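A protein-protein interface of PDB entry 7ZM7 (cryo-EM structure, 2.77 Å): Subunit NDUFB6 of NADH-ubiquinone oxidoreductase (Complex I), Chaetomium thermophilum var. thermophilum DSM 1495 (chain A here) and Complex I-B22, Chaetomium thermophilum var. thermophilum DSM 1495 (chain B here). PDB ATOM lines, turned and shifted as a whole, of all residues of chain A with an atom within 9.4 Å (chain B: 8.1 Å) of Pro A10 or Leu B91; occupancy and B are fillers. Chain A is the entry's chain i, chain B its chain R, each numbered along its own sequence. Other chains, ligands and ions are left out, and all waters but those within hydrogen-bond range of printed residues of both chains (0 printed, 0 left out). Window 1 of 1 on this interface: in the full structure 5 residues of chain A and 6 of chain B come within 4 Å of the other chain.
Of the printed residues of chain B, Tyr A9 touches Leu B91 (3.7 Å). Pro A10 touches just these residues of chain B: Val B88 (3.7 Å) and Leu B91 (3.6 Å). Of the printed residues of chain B, His A12 touches Glu B92 and Pro B94. Gly A19 touches none of the printed residues of chain B. Of the printed residues of chain A, Pro B87 touches Ile A7 and Pro A8. No residue of chain A comes within 4 Å of Asn B90. Glu B92 touches just one residue of chain A: His A12. The nearest residue of chain A that does not touch Leu B91 is Pro A8 (4.1 Å).
Ile A7 touches Pro B87 (CG2 to CB, 3.98 Å). Pro B87 touches Pro A8 (CB to O, 3.7 Å). CD2 of Leu B91 touches C of Tyr A9, at 3.7 Å. CD of Pro A10 touches CG2 of Val B88 (3.7 Å). Pro A10 touches Leu B91 (N to CD2, 3.6 Å). Glu B92 touches His A12. His A12 touches Pro B94.
The side-chain amide oxygen of Asn B90 lies close to the side-chain carboxylate of Glu B92 (3.0 Å). The side-chain hydroxyl (OH) of Tyr A9 lies close to the side-chain amino group (NZ) of Lys A11 (3.4 Å).
Printed residues of chain A that touch a printed residue of chain B: Ile A7, Pro A8, Tyr A9, Pro A10 and His A12. Hydrophobic or aromatic side chains of chain B that line the printed part of chain A: Pro B87, Val B88, Leu B91 and Pro B94. Among the printed residues, no Asp or Glu carboxylate lies within 4 Å of a Lys or Arg side-chain nitrogen of the other chain.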
ATOM      1  N   LYS A   6     -34.521 -21.477 -23.078  1.00  0.00           N
ATOM      2  CA  LYS A   6     -34.154 -21.857 -21.725  1.00  0.00           C
ATOM      3  C   LYS A   6     -33.245 -20.811 -21.100  1.00  0.00           C
ATOM      4  O   LYS A   6     -32.344 -20.273 -21.749  1.00  0.00           O
ATOM      5  CB  LYS A   6     -33.480 -23.221 -21.762  1.00  0.00           C
ATOM      6  CG  LYS A   6     -34.461 -24.309 -22.117  1.00  0.00           C
ATOM      7  CD  LYS A   6     -33.797 -25.634 -22.319  1.00  0.00           C
ATOM      8  CE  LYS A   6     -33.289 -26.235 -21.076  1.00  0.00           C
ATOM      9  NZ  LYS A   6     -32.768 -27.575 -21.390  1.00  0.00           N
ATOM     10  N   ILE A   7     -33.488 -20.526 -19.832  1.00  0.00           N
ATOM     11  CA  ILE A   7     -32.768 -19.467 -19.124  1.00  0.00           C
ATOM     12  C   ILE A   7     -31.298 -19.849 -19.018  1.00  0.00           C
ATOM     13  O   ILE A   7     -30.985 -21.036 -18.824  1.00  0.00           O
ATOM     14  CB  ILE A   7     -33.380 -19.256 -17.737  1.00  0.00           C
ATOM     15  CG1 ILE A   7     -34.904 -19.130 -17.832  1.00  0.00           C
ATOM     16  CG2 ILE A   7     -32.769 -18.079 -17.044  1.00  0.00           C
ATOM     17  CD1 ILE A   7     -35.377 -17.921 -18.543  1.00  0.00           C
ATOM     18  N   PRO A   8     -30.368 -18.914 -19.174  1.00  0.00           N
ATOM     19  CA  PRO A   8     -28.980 -19.204 -18.822  1.00  0.00           C
ATOM     20  C   PRO A   8     -28.824 -19.293 -17.316  1.00  0.00           C
ATOM     21  O   PRO A   8     -29.421 -18.521 -16.570  1.00  0.00           O
ATOM     22  CB  PRO A   8     -28.213 -18.009 -19.394  1.00  0.00           C
ATOM     23  CG  PRO A   8     -29.204 -16.934 -19.454  1.00  0.00           C
ATOM     24  CD  PRO A   8     -30.515 -17.576 -19.762  1.00  0.00           C
ATOM     25  N   TYR A   9     -28.015 -20.239 -16.866  1.00  0.00           N
ATOM     26  CA  TYR A   9     -27.838 -20.440 -15.438  1.00  0.00           C
ATOM     27  C   TYR A   9     -26.396 -20.824 -15.178  1.00  0.00           C
ATOM     28  O   TYR A   9     -25.693 -21.258 -16.092  1.00  0.00           O
ATOM     29  CB  TYR A   9     -28.782 -21.515 -14.886  1.00  0.00           C
ATOM     30  CG  TYR A   9     -28.676 -22.855 -15.542  1.00  0.00           C
ATOM     31  CD1 TYR A   9     -29.232 -23.092 -16.784  1.00  0.00           C
ATOM     32  CD2 TYR A   9     -28.018 -23.890 -14.910  1.00  0.00           C
ATOM     33  CE1 TYR A   9     -29.138 -24.322 -17.374  1.00  0.00           C
ATOM     34  CE2 TYR A   9     -27.910 -25.119 -15.496  1.00  0.00           C
ATOM     35  CZ  TYR A   9     -28.470 -25.333 -16.724  1.00  0.00           C
ATOM     36  OH  TYR A   9     -28.359 -26.572 -17.296  1.00  0.00           O
ATOM     37  N   PRO A  10     -25.916 -20.643 -13.949  1.00  0.00           N
ATOM     38  CA  PRO A  10     -24.573 -21.108 -13.609  1.00  0.00           C
ATOM     39  C   PRO A  10     -24.556 -22.607 -13.387  1.00  0.00           C
ATOM     40  O   PRO A  10     -25.415 -23.164 -12.703  1.00  0.00           O
ATOM     41  CB  PRO A  10     -24.265 -20.348 -12.320  1.00  0.00           C
ATOM     42  CG  PRO A  10     -25.586 -20.198 -11.700  1.00  0.00           C
ATOM     43  CD  PRO A  10     -26.564 -19.992 -12.800  1.00  0.00           C
ATOM     44  N   LYS A  11     -23.553 -23.260 -13.955  1.00  0.00           N
ATOM     45  CA  LYS A  11     -23.466 -24.709 -13.911  1.00  0.00           C
ATOM     46  C   LYS A  11     -22.733 -25.236 -12.683  1.00  0.00           C
ATOM     47  O   LYS A  11     -22.629 -26.449 -12.520  1.00  0.00           O
ATOM     48  CB  LYS A  11     -22.790 -25.217 -15.174  1.00  0.00           C
ATOM     49  CG  LYS A  11     -23.241 -24.512 -16.444  1.00  0.00           C
ATOM     50  CD  LYS A  11     -24.673 -24.826 -16.815  1.00  0.00           C
ATOM     51  CE  LYS A  11     -24.860 -24.790 -18.327  1.00  0.00           C
ATOM     52  NZ  LYS A  11     -26.221 -24.335 -18.767  1.00  0.00           N
ATOM     53  N   HIS A  12     -22.233 -24.365 -11.815  1.00  0.00           N
ATOM     54  CA  HIS A  12     -21.535 -24.803 -10.619  1.00  0.00           C
ATOM     55  C   HIS A  12     -22.453 -24.984  -9.425  1.00  0.00           C
ATOM     56  O   HIS A  12     -21.999 -25.468  -8.391  1.00  0.00           O
ATOM     57  CB  HIS A  12     -20.431 -23.815 -10.258  1.00  0.00           C
ATOM     58  CG  HIS A  12     -20.926 -22.523  -9.701  1.00  0.00           C
ATOM     59  ND1 HIS A  12     -21.524 -21.562 -10.479  1.00  0.00           N
ATOM     60  CD2 HIS A  12     -20.894 -22.026  -8.444  1.00  0.00           C
ATOM     61  CE1 HIS A  12     -21.847 -20.531  -9.722  1.00  0.00           C
ATOM     62  NE2 HIS A  12     -21.476 -20.787  -8.483  1.00  0.00           N
ATOM     63  N   VAL A  13     -23.725 -24.634  -9.543  1.00  0.00           N
ATOM     64  CA  VAL A  13     -24.633 -24.619  -8.406  1.00  0.00           C
ATOM     65  C   VAL A  13     -25.245 -26.002  -8.236  1.00  0.00           C
ATOM     66  O   VAL A  13     -25.808 -26.565  -9.178  1.00  0.00           O
ATOM     67  CB  VAL A  13     -25.719 -23.549  -8.579  1.00  0.00           C
ATOM     68  CG1 VAL A  13     -26.777 -23.707  -7.523  1.00  0.00           C
ATOM     69  CG2 VAL A  13     -25.106 -22.168  -8.514  1.00  0.00           C
ATOM     70  N   TRP A  14     -25.142 -26.546  -7.031  1.00  0.00           N
ATOM     71  CA  TRP A  14     -25.663 -27.862  -6.708  1.00  0.00           C
ATOM     72  C   TRP A  14     -26.947 -27.696  -5.909  1.00  0.00           C
ATOM     73  O   TRP A  14     -26.973 -26.960  -4.924  1.00  0.00           O
ATOM     74  CB  TRP A  14     -24.634 -28.673  -5.921  1.00  0.00           C
ATOM     75  CG  TRP A  14     -25.025 -30.100  -5.741  1.00  0.00           C
ATOM     76  CD1 TRP A  14     -24.607 -31.159  -6.482  1.00  0.00           C
ATOM     77  CD2 TRP A  14     -25.920 -30.628  -4.760  1.00  0.00           C
ATOM     78  NE1 TRP A  14     -25.176 -32.308  -6.023  1.00  0.00           N
ATOM     79  CE2 TRP A  14     -25.997 -32.011  -4.971  1.00  0.00           C
ATOM     80  CE3 TRP A  14     -26.669 -30.063  -3.728  1.00  0.00           C
ATOM     81  CZ2 TRP A  14     -26.784 -32.839  -4.188  1.00  0.00           C
ATOM     82  CZ3 TRP A  14     -27.454 -30.887  -2.956  1.00  0.00           C
ATOM     83  CH2 TRP A  14     -27.509 -32.261  -3.195  1.00  0.00           C
ATOM     84  N   SER A  15     -28.004 -28.386  -6.320  1.00  0.00           N
ATOM     85  CA  SER A  15     -29.294 -28.249  -5.674  1.00  0.00           C
ATOM     86  C   SER A  15     -29.951 -29.616  -5.525  1.00  0.00           C
ATOM     87  O   SER A  15     -29.987 -30.384  -6.490  1.00  0.00           O
ATOM     88  CB  SER A  15     -30.191 -27.317  -6.479  1.00  0.00           C
ATOM     89  OG  SER A  15     -31.527 -27.460  -6.072  1.00  0.00           O
ATOM     90  N   GLY A  18     -32.614 -30.559  -8.219  1.00  0.00           N
ATOM     91  CA  GLY A  18     -32.235 -30.523  -9.610  1.00  0.00           C
ATOM     92  C   GLY A  18     -31.639 -29.209 -10.049  1.00  0.00           C
ATOM     93  O   GLY A  18     -30.638 -29.179 -10.760  1.00  0.00           O
ATOM     94  N   GLY A  19     -32.219 -28.113  -9.622  1.00  0.00           N
ATOM     95  CA  GLY A  19     -31.824 -26.815 -10.133  1.00  0.00           C
ATOM     96  C   GLY A  19     -32.583 -26.500 -11.400  1.00  0.00           C
ATOM     97  O   GLY A  19     -33.806 -26.594 -11.432  1.00  0.00           O
ATOM     98  N   TRP A  20     -31.853 -26.156 -12.455  1.00  0.00           N
ATOM     99  CA  TRP A  20     -32.448 -25.734 -13.713  1.00  0.00           C
ATOM    100  C   TRP A  20     -32.513 -26.913 -14.677  1.00  0.00           C
ATOM    101  O   TRP A  20     -31.484 -27.502 -15.007  1.00  0.00           O
ATOM    102  CB  TRP A  20     -31.652 -24.587 -14.327  1.00  0.00           C
ATOM    103  CG  TRP A  20     -31.700 -23.256 -13.614  1.00  0.00           C
ATOM    104  CD1 TRP A  20     -32.505 -22.215 -13.913  1.00  0.00           C
ATOM    105  CD2 TRP A  20     -30.889 -22.824 -12.516  1.00  0.00           C
ATOM    106  NE1 TRP A  20     -32.264 -21.166 -13.073  1.00  0.00           N
ATOM    107  CE2 TRP A  20     -31.271 -21.518 -12.207  1.00  0.00           C
ATOM    108  CE3 TRP A  20     -29.874 -23.414 -11.772  1.00  0.00           C
ATOM    109  CZ2 TRP A  20     -30.681 -20.797 -11.185  1.00  0.00           C
ATOM    110  CZ3 TRP A  20     -29.297 -22.696 -10.756  1.00  0.00           C
ATOM    111  CH2 TRP A  20     -29.694 -21.401 -10.479  1.00  0.00           C
ATOM    112  N   PRO B  87     -32.328 -14.304 -14.639  1.00  0.00           N
ATOM    113  CA  PRO B  87     -31.116 -15.117 -14.530  1.00  0.00           C
ATOM    114  C   PRO B  87     -30.185 -14.571 -13.469  1.00  0.00           C
ATOM    115  O   PRO B  87     -30.295 -13.426 -13.038  1.00  0.00           O
ATOM    116  CB  PRO B  87     -30.490 -15.010 -15.921  1.00  0.00           C
ATOM    117  CG  PRO B  87     -31.041 -13.751 -16.482  1.00  0.00           C
ATOM    118  CD  PRO B  87     -32.425 -13.637 -15.946  1.00  0.00           C
ATOM    119  N   VAL B  88     -29.270 -15.424 -13.033  1.00  0.00           N
ATOM    120  CA  VAL B  88     -28.200 -14.954 -12.150  1.00  0.00           C
ATOM    121  C   VAL B  88     -27.351 -13.941 -12.907  1.00  0.00           C
ATOM    122  O   VAL B  88     -27.051 -14.150 -14.095  1.00  0.00           O
ATOM    123  CB  VAL B  88     -27.352 -16.140 -11.650  1.00  0.00           C
ATOM    124  CG1 VAL B  88     -26.335 -15.685 -10.640  1.00  0.00           C
ATOM    125  CG2 VAL B  88     -28.239 -17.213 -11.050  1.00  0.00           C
ATOM    126  N   PRO B  89     -26.991 -12.824 -12.316  1.00  0.00           N
ATOM    127  CA  PRO B  89     -26.217 -11.817 -13.048  1.00  0.00           C
ATOM    128  C   PRO B  89     -24.729 -12.119 -13.106  1.00  0.00           C
ATOM    129  O   PRO B  89     -23.931 -11.251 -13.454  1.00  0.00           O
ATOM    130  CB  PRO B  89     -26.485 -10.529 -12.255  1.00  0.00           C
ATOM    131  CG  PRO B  89     -27.587 -10.858 -11.296  1.00  0.00           C
ATOM    132  CD  PRO B  89     -27.498 -12.300 -11.039  1.00  0.00           C
ATOM    133  N   ASN B  90     -24.347 -13.338 -12.766  1.00  0.00           N
ATOM    134  CA  ASN B  90     -22.945 -13.721 -12.661  1.00  0.00           C
ATOM    135  C   ASN B  90     -22.897 -15.239 -12.731  1.00  0.00           C
ATOM    136  O   ASN B  90     -23.222 -15.910 -11.750  1.00  0.00           O
ATOM    137  CB  ASN B  90     -22.344 -13.210 -11.354  1.00  0.00           C
ATOM    138  CG  ASN B  90     -20.856 -13.435 -11.251  1.00  0.00           C
ATOM    139  OD1 ASN B  90     -20.330 -14.432 -11.716  1.00  0.00           O
ATOM    140  ND2 ASN B  90     -20.178 -12.518 -10.592  1.00  0.00           N
ATOM    141  N   LEU B  91     -22.495 -15.782 -13.872  1.00  0.00           N
ATOM    142  CA  LEU B  91     -22.498 -17.221 -14.059  1.00  0.00           C
ATOM    143  C   LEU B  91     -21.115 -17.839 -13.981  1.00  0.00           C
ATOM    144  O   LEU B  91     -20.992 -19.057 -14.136  1.00  0.00           O
ATOM    145  CB  LEU B  91     -23.122 -17.587 -15.410  1.00  0.00           C
ATOM    146  CG  LEU B  91     -24.441 -16.997 -15.882  1.00  0.00           C
ATOM    147  CD1 LEU B  91     -24.772 -17.642 -17.203  1.00  0.00           C
ATOM    148  CD2 LEU B  91     -25.566 -17.211 -14.893  1.00  0.00           C
ATOM    149  N   GLU B  92     -20.076 -17.043 -13.786  1.00  0.00           N
ATOM    150  CA  GLU B  92     -18.749 -17.607 -13.665  1.00  0.00           C
ATOM    151  C   GLU B  92     -18.621 -18.376 -12.354  1.00  0.00           C
ATOM    152  O   GLU B  92     -19.237 -18.015 -11.347  1.00  0.00           O
ATOM    153  CB  GLU B  92     -17.687 -16.515 -13.738  1.00  0.00           C
ATOM    154  CG  GLU B  92     -17.534 -15.891 -15.112  1.00  0.00           C
ATOM    155  CD  GLU B  92     -18.555 -14.807 -15.399  1.00  0.00           C
ATOM    156  OE1 GLU B  92     -19.361 -14.485 -14.503  1.00  0.00           O
ATOM    157  OE2 GLU B  92     -18.548 -14.274 -16.529  1.00  0.00           O
ATOM    158  N   PRO B  93     -17.879 -19.517 -12.337  1.00  0.00           N
ATOM    159  CA  PRO B  93     -17.632 -20.234 -11.099  1.00  0.00           C
ATOM    160  C   PRO B  93     -17.009 -19.251 -10.105  1.00  0.00           C
ATOM    161  O   PRO B  93     -16.326 -18.342 -10.526  1.00  0.00           O
ATOM    162  CB  PRO B  93     -16.553 -21.232 -11.508  1.00  0.00           C
ATOM    163  CG  PRO B  93     -16.950 -21.615 -12.895  1.00  0.00           C
ATOM    164  CD  PRO B  93     -17.315 -20.274 -13.485  1.00  0.00           C
ATOM    165  N   PRO B  94     -17.194 -19.447  -8.785  1.00  0.00           N
ATOM    166  CA  PRO B  94     -16.673 -18.507  -7.802  1.00  0.00           C
ATOM    167  C   PRO B  94     -15.142 -18.634  -7.730  1.00  0.00           C
ATOM    168  O   PRO B  94     -14.631 -19.666  -8.099  1.00  0.00           O
ATOM    169  CB  PRO B  94     -17.369 -18.964  -6.509  1.00  0.00           C
ATOM    170  CG  PRO B  94     -18.406 -19.976  -6.924  1.00  0.00           C
ATOM    171  CD  PRO B  94     -17.847 -20.599  -8.179  1.00  0.00           C
